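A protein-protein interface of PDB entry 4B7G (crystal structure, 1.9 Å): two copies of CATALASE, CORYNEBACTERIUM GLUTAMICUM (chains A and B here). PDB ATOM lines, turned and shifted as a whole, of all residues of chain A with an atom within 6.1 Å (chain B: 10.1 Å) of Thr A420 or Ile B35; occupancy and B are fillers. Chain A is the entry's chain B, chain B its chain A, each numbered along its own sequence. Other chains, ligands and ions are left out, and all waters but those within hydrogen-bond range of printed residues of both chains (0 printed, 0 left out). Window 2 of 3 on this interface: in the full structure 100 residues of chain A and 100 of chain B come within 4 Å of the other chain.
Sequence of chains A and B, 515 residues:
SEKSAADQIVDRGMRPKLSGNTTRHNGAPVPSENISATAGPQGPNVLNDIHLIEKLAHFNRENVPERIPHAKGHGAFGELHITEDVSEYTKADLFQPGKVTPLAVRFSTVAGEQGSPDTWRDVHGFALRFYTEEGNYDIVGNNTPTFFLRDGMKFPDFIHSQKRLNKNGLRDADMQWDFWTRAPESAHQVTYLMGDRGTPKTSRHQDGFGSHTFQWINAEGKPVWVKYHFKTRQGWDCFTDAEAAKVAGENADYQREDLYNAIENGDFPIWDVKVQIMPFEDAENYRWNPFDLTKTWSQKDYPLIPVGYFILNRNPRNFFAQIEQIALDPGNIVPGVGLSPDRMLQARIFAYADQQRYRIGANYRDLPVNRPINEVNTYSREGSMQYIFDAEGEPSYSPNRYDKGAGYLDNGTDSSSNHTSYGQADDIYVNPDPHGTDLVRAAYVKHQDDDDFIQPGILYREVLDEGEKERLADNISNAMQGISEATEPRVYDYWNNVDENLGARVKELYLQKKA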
ATOM      1  N   ASP A 410       0.122  10.130  10.115  1.00  0.00           N
ATOM      2  CA  ASP A 410       1.185  10.114   9.109  1.00  0.00           C
ATOM      3  C   ASP A 410       2.239  11.161   9.460  1.00  0.00           C
ATOM      4  O   ASP A 410       2.021  11.990  10.348  1.00  0.00           O
ATOM      5  CB  ASP A 410       0.608  10.449   7.728  1.00  0.00           C
ATOM      6  CG  ASP A 410      -0.577   9.579   7.350  1.00  0.00           C
ATOM      7  OD1 ASP A 410      -0.574   8.370   7.673  1.00  0.00           O
ATOM      8  OD2 ASP A 410      -1.519  10.104   6.712  1.00  0.00           O
ATOM      9  N   ASP A 414       5.983  11.057   3.703  1.00  0.00           N
ATOM     10  CA  ASP A 414       6.064   9.794   2.964  1.00  0.00           C
ATOM     11  C   ASP A 414       4.796   8.942   3.109  1.00  0.00           C
ATOM     12  O   ASP A 414       3.826   9.353   3.752  1.00  0.00           O
ATOM     13  CB  ASP A 414       7.329   8.990   3.338  1.00  0.00           C
ATOM     14  CG  ASP A 414       7.359   8.577   4.795  1.00  0.00           C
ATOM     15  OD1 ASP A 414       6.332   8.086   5.327  1.00  0.00           O
ATOM     16  OD2 ASP A 414       8.425   8.743   5.421  1.00  0.00           O
ATOM     17  N   SER A 415       4.827   7.755   2.514  1.00  0.00           N
ATOM     18  CA  SER A 415       3.657   6.884   2.430  1.00  0.00           C
ATOM     19  C   SER A 415       3.509   5.888   3.583  1.00  0.00           C
ATOM     20  O   SER A 415       2.680   4.976   3.496  1.00  0.00           O
ATOM     21  CB  SER A 415       3.734   6.092   1.132  1.00  0.00           C
ATOM     22  OG  SER A 415       4.884   5.261   1.145  1.00  0.00           O
ATOM     23  N   SER A 416       4.302   6.047   4.648  1.00  0.00           N
ATOM     24  CA  SER A 416       4.269   5.125   5.795  1.00  0.00           C
ATOM     25  C   SER A 416       4.627   3.696   5.396  1.00  0.00           C
ATOM     26  O   SER A 416       4.069   2.727   5.929  1.00  0.00           O
ATOM     27  CB  SER A 416       2.910   5.163   6.514  1.00  0.00           C
ATOM     28  OG  SER A 416       2.579   6.498   6.902  1.00  0.00           O
ATOM     29  N   SER A 417       5.569   3.561   4.469  1.00  0.00           N
ATOM     30  CA  SER A 417       6.088   2.240   4.122  1.00  0.00           C
ATOM     31  C   SER A 417       7.101   1.825   5.189  1.00  0.00           C
ATOM     32  O   SER A 417       7.043   2.322   6.318  1.00  0.00           O
ATOM     33  CB  SER A 417       6.715   2.264   2.730  1.00  0.00           C
ATOM     34  OG  SER A 417       7.067   0.960   2.296  1.00  0.00           O
ATOM     35  N   ASN A 418       8.023   0.926   4.839  1.00  0.00           N
ATOM     36  CA  ASN A 418       9.016   0.423   5.795  1.00  0.00           C
ATOM     37  C   ASN A 418       8.352  -0.214   7.007  1.00  0.00           C
ATOM     38  O   ASN A 418       8.821  -0.064   8.144  1.00  0.00           O
ATOM     39  CB  ASN A 418       9.967   1.545   6.226  1.00  0.00           C
ATOM     40  CG  ASN A 418      10.505   2.331   5.042  1.00  0.00           C
ATOM     41  OD1 ASN A 418      11.221   1.783   4.212  1.00  0.00           O
ATOM     42  ND2 ASN A 418      10.165   3.620   4.963  1.00  0.00           N
ATOM     43  N   HIS A 419       7.389  -0.757   6.759  1.00  0.00           N
ATOM     44  CA  HIS A 419       6.507  -1.420   7.715  1.00  0.00           C
ATOM     45  C   HIS A 419       6.094  -0.576   8.919  1.00  0.00           C
ATOM     46  O   HIS A 419       6.238  -0.989  10.067  1.00  0.00           O
ATOM     47  CB  HIS A 419       7.107  -2.762   8.134  1.00  0.00           C
ATOM     48  CG  HIS A 419       7.173  -3.742   7.008  1.00  0.00           C
ATOM     49  ND1 HIS A 419       8.198  -3.750   6.087  1.00  0.00           N
ATOM     50  CD2 HIS A 419       6.377  -4.794   6.692  1.00  0.00           C
ATOM     51  CE1 HIS A 419       8.015  -4.743   5.233  1.00  0.00           C
ATOM     52  NE2 HIS A 419       6.915  -5.389   5.577  1.00  0.00           N
ATOM     53  N   THR A 420       5.524   0.488   8.686  1.00  0.00           N
ATOM     54  CA  THR A 420       4.988   1.382   9.702  1.00  0.00           C
ATOM     55  C   THR A 420       3.614   0.891  10.154  1.00  0.00           C
ATOM     56  O   THR A 420       2.779   0.551   9.318  1.00  0.00           O
ATOM     57  CB  THR A 420       4.845   2.800   9.133  1.00  0.00           C
ATOM     58  OG1 THR A 420       6.138   3.286   8.738  1.00  0.00           O
ATOM     59  CG2 THR A 420       4.235   3.752  10.176  1.00  0.00           C
ATOM     60  N   SER A 421       3.391   0.835  11.467  1.00  0.00           N
ATOM     61  CA  SER A 421       2.082   0.474  12.019  1.00  0.00           C
ATOM     62  C   SER A 421       1.616   1.546  12.991  1.00  0.00           C
ATOM     63  O   SER A 421       2.436   2.147  13.694  1.00  0.00           O
ATOM     64  CB  SER A 421       2.147  -0.871  12.742  1.00  0.00           C
ATOM     65  OG  SER A 421       2.471  -1.923  11.850  1.00  0.00           O
ATOM     66  N   TYR A 422       0.306   1.784  13.041  1.00  0.00           N
ATOM     67  CA  TYR A 422      -0.245   2.798  13.936  1.00  0.00           C
ATOM     68  C   TYR A 422      -0.998   2.213  15.133  1.00  0.00           C
ATOM     69  O   TYR A 422      -1.183   2.892  16.152  1.00  0.00           O
ATOM     70  CB  TYR A 422      -1.193   3.724  13.169  1.00  0.00           C
ATOM     71  CG  TYR A 422      -0.542   4.533  12.060  1.00  0.00           C
ATOM     72  CD1 TYR A 422       0.752   5.048  12.194  1.00  0.00           C
ATOM     73  CD2 TYR A 422      -1.230   4.784  10.878  1.00  0.00           C
ATOM     74  CE1 TYR A 422       1.338   5.808  11.163  1.00  0.00           C
ATOM     75  CE2 TYR A 422      -0.662   5.536   9.857  1.00  0.00           C
ATOM     76  CZ  TYR A 422       0.609   6.043   9.999  1.00  0.00           C
ATOM     77  OH  TYR A 422       1.135   6.782   8.959  1.00  0.00           O
ATOM     78  N   VAL B  30      -8.542  13.498   9.776  1.00  0.00           N
ATOM     79  CA  VAL B  30      -8.240  12.237   9.086  1.00  0.00           C
ATOM     80  C   VAL B  30      -7.106  11.528   9.815  1.00  0.00           C
ATOM     81  O   VAL B  30      -6.088  12.150  10.102  1.00  0.00           O
ATOM     82  CB  VAL B  30      -7.792  12.475   7.628  1.00  0.00           C
ATOM     83  CG1 VAL B  30      -7.155  11.207   7.051  1.00  0.00           C
ATOM     84  CG2 VAL B  30      -8.968  12.928   6.760  1.00  0.00           C
ATOM     85  N   PRO B  31      -7.272  10.231  10.130  1.00  0.00           N
ATOM     86  CA  PRO B  31      -6.146   9.564  10.797  1.00  0.00           C
ATOM     87  C   PRO B  31      -4.995   9.274   9.830  1.00  0.00           C
ATOM     88  O   PRO B  31      -3.848   9.627  10.129  1.00  0.00           O
ATOM     89  CB  PRO B  31      -6.764   8.260  11.329  1.00  0.00           C
ATOM     90  CG  PRO B  31      -8.237   8.546  11.427  1.00  0.00           C
ATOM     91  CD  PRO B  31      -8.521   9.455  10.246  1.00  0.00           C
ATOM     92  N   SER B  32      -5.280   8.679   8.676  1.00  0.00           N
ATOM     93  CA  SER B  32      -4.199   8.386   7.733  1.00  0.00           C
ATOM     94  C   SER B  32      -4.617   8.553   6.285  1.00  0.00           C
ATOM     95  O   SER B  32      -5.748   8.212   5.913  1.00  0.00           O
ATOM     96  CB  SER B  32      -3.698   6.958   7.941  1.00  0.00           C
ATOM     97  OG  SER B  32      -2.622   6.657   7.069  1.00  0.00           O
ATOM     98  N   GLU B  33      -3.704   9.065   5.462  1.00  0.00           N
ATOM     99  CA  GLU B  33      -3.916   9.074   4.016  1.00  0.00           C
ATOM    100  C   GLU B  33      -3.159   7.924   3.371  1.00  0.00           C
ATOM    101  O   GLU B  33      -3.120   7.825   2.139  1.00  0.00           O
ATOM    102  CB  GLU B  33      -3.405  10.378   3.394  1.00  0.00           C
ATOM    103  CG  GLU B  33      -4.100  11.640   3.861  1.00  0.00           C
ATOM    104  CD  GLU B  33      -5.520  11.765   3.348  1.00  0.00           C
ATOM    105  OE1 GLU B  33      -5.998  10.855   2.618  1.00  0.00           O
ATOM    106  OE2 GLU B  33      -6.167  12.784   3.680  1.00  0.00           O
ATOM    107  N   ASN B  34      -2.565   7.055   4.194  1.00  0.00           N
ATOM    108  CA  ASN B  34      -1.660   6.009   3.703  1.00  0.00           C
ATOM    109  C   ASN B  34      -2.110   4.568   3.958  1.00  0.00           C
ATOM    110  O   ASN B  34      -1.833   3.672   3.151  1.00  0.00           O
ATOM    111  CB  ASN B  34      -0.260   6.201   4.317  1.00  0.00           C
ATOM    112  CG  ASN B  34       0.397   7.509   3.894  1.00  0.00           C
ATOM    113  OD1 ASN B  34       0.099   8.046   2.826  1.00  0.00           O
ATOM    114  ND2 ASN B  34       1.304   8.023   4.729  1.00  0.00           N
ATOM    115  N   ILE B  35      -2.773   4.338   5.090  1.00  0.00           N
ATOM    116  CA  ILE B  35      -3.065   2.977   5.535  1.00  0.00           C
ATOM    117  C   ILE B  35      -4.540   2.839   5.898  1.00  0.00           C
ATOM    118  O   ILE B  35      -5.082   3.674   6.632  1.00  0.00           O
ATOM    119  CB  ILE B  35      -2.204   2.596   6.778  1.00  0.00           C
ATOM    120  CG1 ILE B  35      -0.708   2.811   6.492  1.00  0.00           C
ATOM    121  CG2 ILE B  35      -2.480   1.165   7.204  1.00  0.00           C
ATOM    122  CD1 ILE B  35       0.209   2.347   7.634  1.00  0.00           C
ATOM    123  N   SER B  36      -5.191   1.796   5.375  1.00  0.00           N
ATOM    124  CA  SER B  36      -6.611   1.543   5.670  1.00  0.00           C
ATOM    125  C   SER B  36      -6.761   0.558   6.820  1.00  0.00           C
ATOM    126  O   SER B  36      -5.848  -0.226   7.100  1.00  0.00           O
ATOM    127  CB  SER B  36      -7.356   1.027   4.436  1.00  0.00           C
ATOM    128  OG  SER B  36      -6.696  -0.090   3.854  1.00  0.00           O
ATOM    129  N   ALA B  37      -7.914   0.603   7.491  1.00  0.00           N
ATOM    130  CA  ALA B  37      -8.136  -0.188   8.709  1.00  0.00           C
ATOM    131  C   ALA B  37      -8.612  -1.612   8.419  1.00  0.00           C
ATOM    132  O   ALA B  37      -9.489  -1.838   7.571  1.00  0.00           O
ATOM    133  CB  ALA B  37      -9.120   0.519   9.623  1.00  0.00           C
ATOM    134  N   THR B  38      -8.043  -2.574   9.147  1.00  0.00           N
ATOM    135  CA  THR B  38      -8.330  -3.987   8.917  1.00  0.00           C
ATOM    136  C   THR B  38      -8.579  -4.684  10.239  1.00  0.00           C
ATOM    137  O   THR B  38      -8.128  -4.211  11.286  1.00  0.00           O
ATOM    138  CB  THR B  38      -7.153  -4.685   8.180  1.00  0.00           C
ATOM    139  OG1 THR B  38      -5.941  -4.521   8.935  1.00  0.00           O
ATOM    140  CG2 THR B  38      -6.952  -4.083   6.782  1.00  0.00           C
ATOM    141  N   GLY B  40      -7.317  -6.908  12.314  1.00  0.00           N
ATOM    142  CA  GLY B  40      -6.010  -7.547  12.396  1.00  0.00           C
ATOM    143  C   GLY B  40      -5.162  -7.148  11.194  1.00  0.00           C
ATOM    144  O   GLY B  40      -5.711  -6.845  10.124  1.00  0.00           O
ATOM    145  N   PRO B  41      -3.826  -7.153  11.346  1.00  0.00           N
ATOM    146  CA  PRO B  41      -2.962  -6.706  10.241  1.00  0.00           C
ATOM    147  C   PRO B  41      -3.196  -7.492   8.951  1.00  0.00           C
ATOM    148  O   PRO B  41      -3.136  -6.909   7.866  1.00  0.00           O
ATOM    149  CB  PRO B  41      -1.548  -6.976  10.770  1.00  0.00           C
ATOM    150  CG  PRO B  41      -1.694  -6.909  12.291  1.00  0.00           C
ATOM    151  CD  PRO B  41      -3.049  -7.534  12.543  1.00  0.00           C
ATOM    152  N   ASN B  45     -10.273  -6.019   5.247  1.00  0.00           N
ATOM    153  CA  ASN B  45     -10.579  -4.608   5.393  1.00  0.00           C
ATOM    154  C   ASN B  45     -11.961  -4.458   6.011  1.00  0.00           C
ATOM    155  O   ASN B  45     -12.899  -5.164   5.627  1.00  0.00           O
ATOM    156  CB  ASN B  45     -10.521  -3.903   4.037  1.00  0.00           C
ATOM    157  CG  ASN B  45      -9.121  -3.422   3.698  1.00  0.00           C
ATOM    158  OD1 ASN B  45      -8.803  -2.232   3.832  1.00  0.00           O
ATOM    159  ND2 ASN B  45      -8.271  -4.349   3.277  1.00  0.00           N
ATOM    160  N   VAL B  46     -12.082  -3.558   6.986  1.00  0.00           N
ATOM    161  CA  VAL B  46     -13.373  -3.293   7.617  1.00  0.00           C
ATOM    162  C   VAL B  46     -14.210  -2.340   6.761  1.00  0.00           C
ATOM    163  O   VAL B  46     -13.674  -1.509   6.019  1.00  0.00           O
ATOM    164  CB  VAL B  46     -13.210  -2.713   9.045  1.00  0.00           C
ATOM    165  CG1 VAL B  46     -12.446  -3.681   9.937  1.00  0.00           C
ATOM    166  CG2 VAL B  46     -12.502  -1.356   9.015  1.00  0.00           C
ATOM    167  N   ASP B  49     -14.063   1.966   7.656  1.00  0.00           N
ATOM    168  CA  ASP B  49     -13.014   2.958   7.457  1.00  0.00           C
ATOM    169  C   ASP B  49     -13.681   4.100   6.698  1.00  0.00           C
ATOM    170  O   ASP B  49     -13.718   4.106   5.467  1.00  0.00           O
ATOM    171  CB  ASP B  49     -11.815   2.392   6.670  1.00  0.00           C
ATOM    172  CG  ASP B  49     -10.624   3.344   6.668  1.00  0.00           C
ATOM    173  OD1 ASP B  49     -10.845   4.580   6.662  1.00  0.00           O
ATOM    174  OD2 ASP B  49      -9.465   2.872   6.689  1.00  0.00           O
ATOM    175  N   ILE B  50     -14.236   5.047   7.448  1.00  0.00           N
ATOM    176  CA  ILE B  50     -15.057   6.107   6.882  1.00  0.00           C
ATOM    177  C   ILE B  50     -14.296   6.932   5.850  1.00  0.00           C
ATOM    178  O   ILE B  50     -14.807   7.177   4.747  1.00  0.00           O
ATOM    179  CB  ILE B  50     -15.619   7.013   8.001  1.00  0.00           C
ATOM    180  CG1 ILE B  50     -16.378   6.167   9.026  1.00  0.00           C
ATOM    181  CG2 ILE B  50     -16.541   8.079   7.428  1.00  0.00           C
ATOM    182  CD1 ILE B  50     -16.873   6.955  10.227  1.00  0.00           C
ATOM    183  N   HIS B  51     -13.072   7.335   6.188  1.00  0.00           N
ATOM    184  CA  HIS B  51     -12.272   8.145   5.269  1.00  0.00           C
ATOM    185  C   HIS B  51     -11.976   7.408   3.971  1.00  0.00           C
ATOM    186  O   HIS B  51     -12.075   7.988   2.883  1.00  0.00           O
ATOM    187  CB  HIS B  51     -10.953   8.574   5.926  1.00  0.00           C
ATOM    188  CG  HIS B  51     -10.094   9.422   5.042  1.00  0.00           C
ATOM    189  ND1 HIS B  51     -10.565  10.560   4.422  1.00  0.00           N
ATOM    190  CD2 HIS B  51      -8.801   9.288   4.654  1.00  0.00           C
ATOM    191  CE1 HIS B  51      -9.595  11.098   3.698  1.00  0.00           C
ATOM    192  NE2 HIS B  51      -8.515  10.345   3.823  1.00  0.00           N
ATOM    193  N   LEU B  52     -11.592   6.137   4.075  1.00  0.00           N
ATOM    194  CA  LEU B  52     -11.271   5.357   2.880  1.00  0.00           C
ATOM    195  C   LEU B  52     -12.428   5.378   1.888  1.00  0.00           C
ATOM    196  O   LEU B  52     -12.237   5.631   0.693  1.00  0.00           O
ATOM    197  CB  LEU B  52     -10.959   3.902   3.244  1.00  0.00           C
ATOM    198  CG  LEU B  52     -10.813   2.956   2.048  1.00  0.00           C
ATOM    199  CD1 LEU B  52      -9.527   3.254   1.253  1.00  0.00           C
ATOM    200  CD2 LEU B  52     -10.849   1.491   2.491  1.00  0.00           C
ATOM    201  N   ILE B  53     -13.635   5.116   2.379  1.00  0.00           N
ATOM    202  CA  ILE B  53     -14.784   5.020   1.482  1.00  0.00           C
ATOM    203  C   ILE B  53     -15.153   6.396   0.918  1.00  0.00           C
ATOM    204  O   ILE B  53     -15.519   6.529  -0.253  1.00  0.00           O
ATOM    205  CB  ILE B  53     -15.994   4.370   2.184  1.00  0.00           C
ATOM    206  CG1 ILE B  53     -15.613   2.975   2.706  1.00  0.00           C
ATOM    207  CG2 ILE B  53     -17.195   4.300   1.227  1.00  0.00           C
ATOM    208  CD1 ILE B  53     -15.173   2.012   1.610  1.00  0.00           C
ATOM    209  N   LYS B  55     -13.076   8.905   0.439  1.00  0.00           N
ATOM    210  CA  LYS B  55     -11.999   9.281  -0.478  1.00  0.00           C
ATOM    211  C   LYS B  55     -12.166   8.557  -1.815  1.00  0.00           C
ATOM    212  O   LYS B  55     -12.049   9.161  -2.886  1.00  0.00           O
ATOM    213  CB  LYS B  55     -10.658   8.907   0.167  1.00  0.00           C
ATOM    214  CG  LYS B  55      -9.393   9.348  -0.593  1.00  0.00           C
ATOM    215  CD  LYS B  55      -8.159   9.215   0.322  1.00  0.00           C
ATOM    216  CE  LYS B  55      -6.867   9.613  -0.400  1.00  0.00           C
ATOM    217  NZ  LYS B  55      -5.639   9.246   0.408  1.00  0.00           N
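Asn B34 touches Asp A410 (ND2 to OD1, 3.5 Å). ND2 of Asn B34 touches C of Ser A415, at 3.3 Å. Thr A420 touches Ile B35 (O to CD1, 3.6 Å). Ser B32 touches Tyr A422. CE2 of Tyr A422 touches CD1 of Ile B35, 3.98 Å away.
OG of Ser B32 is in hydrogen-bond range of OD1 of Asp A410 (2.7 Å). The backbone NH (N) of Glu B33 is in hydrogen-bond range of the side-chain carboxylate (OD2) of Asp A410 (2.7 Å). The backbone carbonyl oxygen (O) of Asp A414 is in hydrogen-bond range of the side-chain amide nitrogen (ND2) of Asn B34. The side-chain hydroxyl (OG) of Ser A416 is in hydrogen-bond range of the side-chain amide nitrogen (ND2) of Asn B34, at 2.9 Å.
Of the printed residues of chain B, Asp A410 touches Ser B32 (2.7 Å), Glu B33 (2.7 Å) and Asn B34 (3.5 Å). Of the printed residues of chain B, Asp A414 touches Asn B34. Of the printed residues of chain B, Ser A415 touches Asn B34 (3.3 Å). Ser A416 touches one residue of chain B. Thr A420 touches just one residue of chain B: Ile B35. No residue of chain B comes within 4 Å of Ser A421. Of the printed residues of chain B, Tyr A422 touches Ser B32 and Ile B35. Of the printed residues of chain A, Glu B33 touches Asp A410. Printed residues of chain A within 4 Å of Ile B35: Thr A420 and Tyr A422. The nearest residue of chain B that does not touch Thr A420 is Asn B34 (7.5 Å). The nearest printed residue of chain A that does not touch Ile B35 is Ser A416 (4.1 Å). The nearest printed residue of chain A that does not touch Glu B33 is Tyr A422 (6.4 Å).
The side-chain hydroxyl of Ser B32 is in hydrogen-bond range of the backbone NH of Asn B34 (2.9 Å). OG of Ser B32 sits at hydrogen-bond distance from N of Ile B35 (3.1 Å). OE1 of Glu B33 sits at hydrogen-bond distance from NE2 of His B51 (2.8 Å). OH of Tyr A422 lies within hydrogen-bond range of OD1 of Asp A410, at 2.7 Å. The side-chain hydroxyl of Ser A416 lies within hydrogen-bond range of the side-chain hydroxyl of Tyr A422, 2.5 Å away. The backbone carbonyl oxygen (O) of Ser A417 lies within hydrogen-bond range of the side-chain hydroxyl (OG1) of Thr A420, 2.8 Å away.
Hydrophobic or aromatic side chains of chain B that line the printed part of chain A: Ile B35. Of the 10 printed residues of chain A, 6 touch a printed residue of chain B. Hydrophobic or aromatic side chains of chain A within 4 Å of the printed part of chain B: Tyr A422. Among the printed residues, 9 pairs touch across the chains. Among the printed residues, no Asp or Glu carboxylate lies within 4 Å of a Lys or Arg side-chain nitrogen of the other chain.
No position is printed for both chains. Of the 9 pairs that touch across the chains among the printed residues, none has its exchanged pair printed and touching as well.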
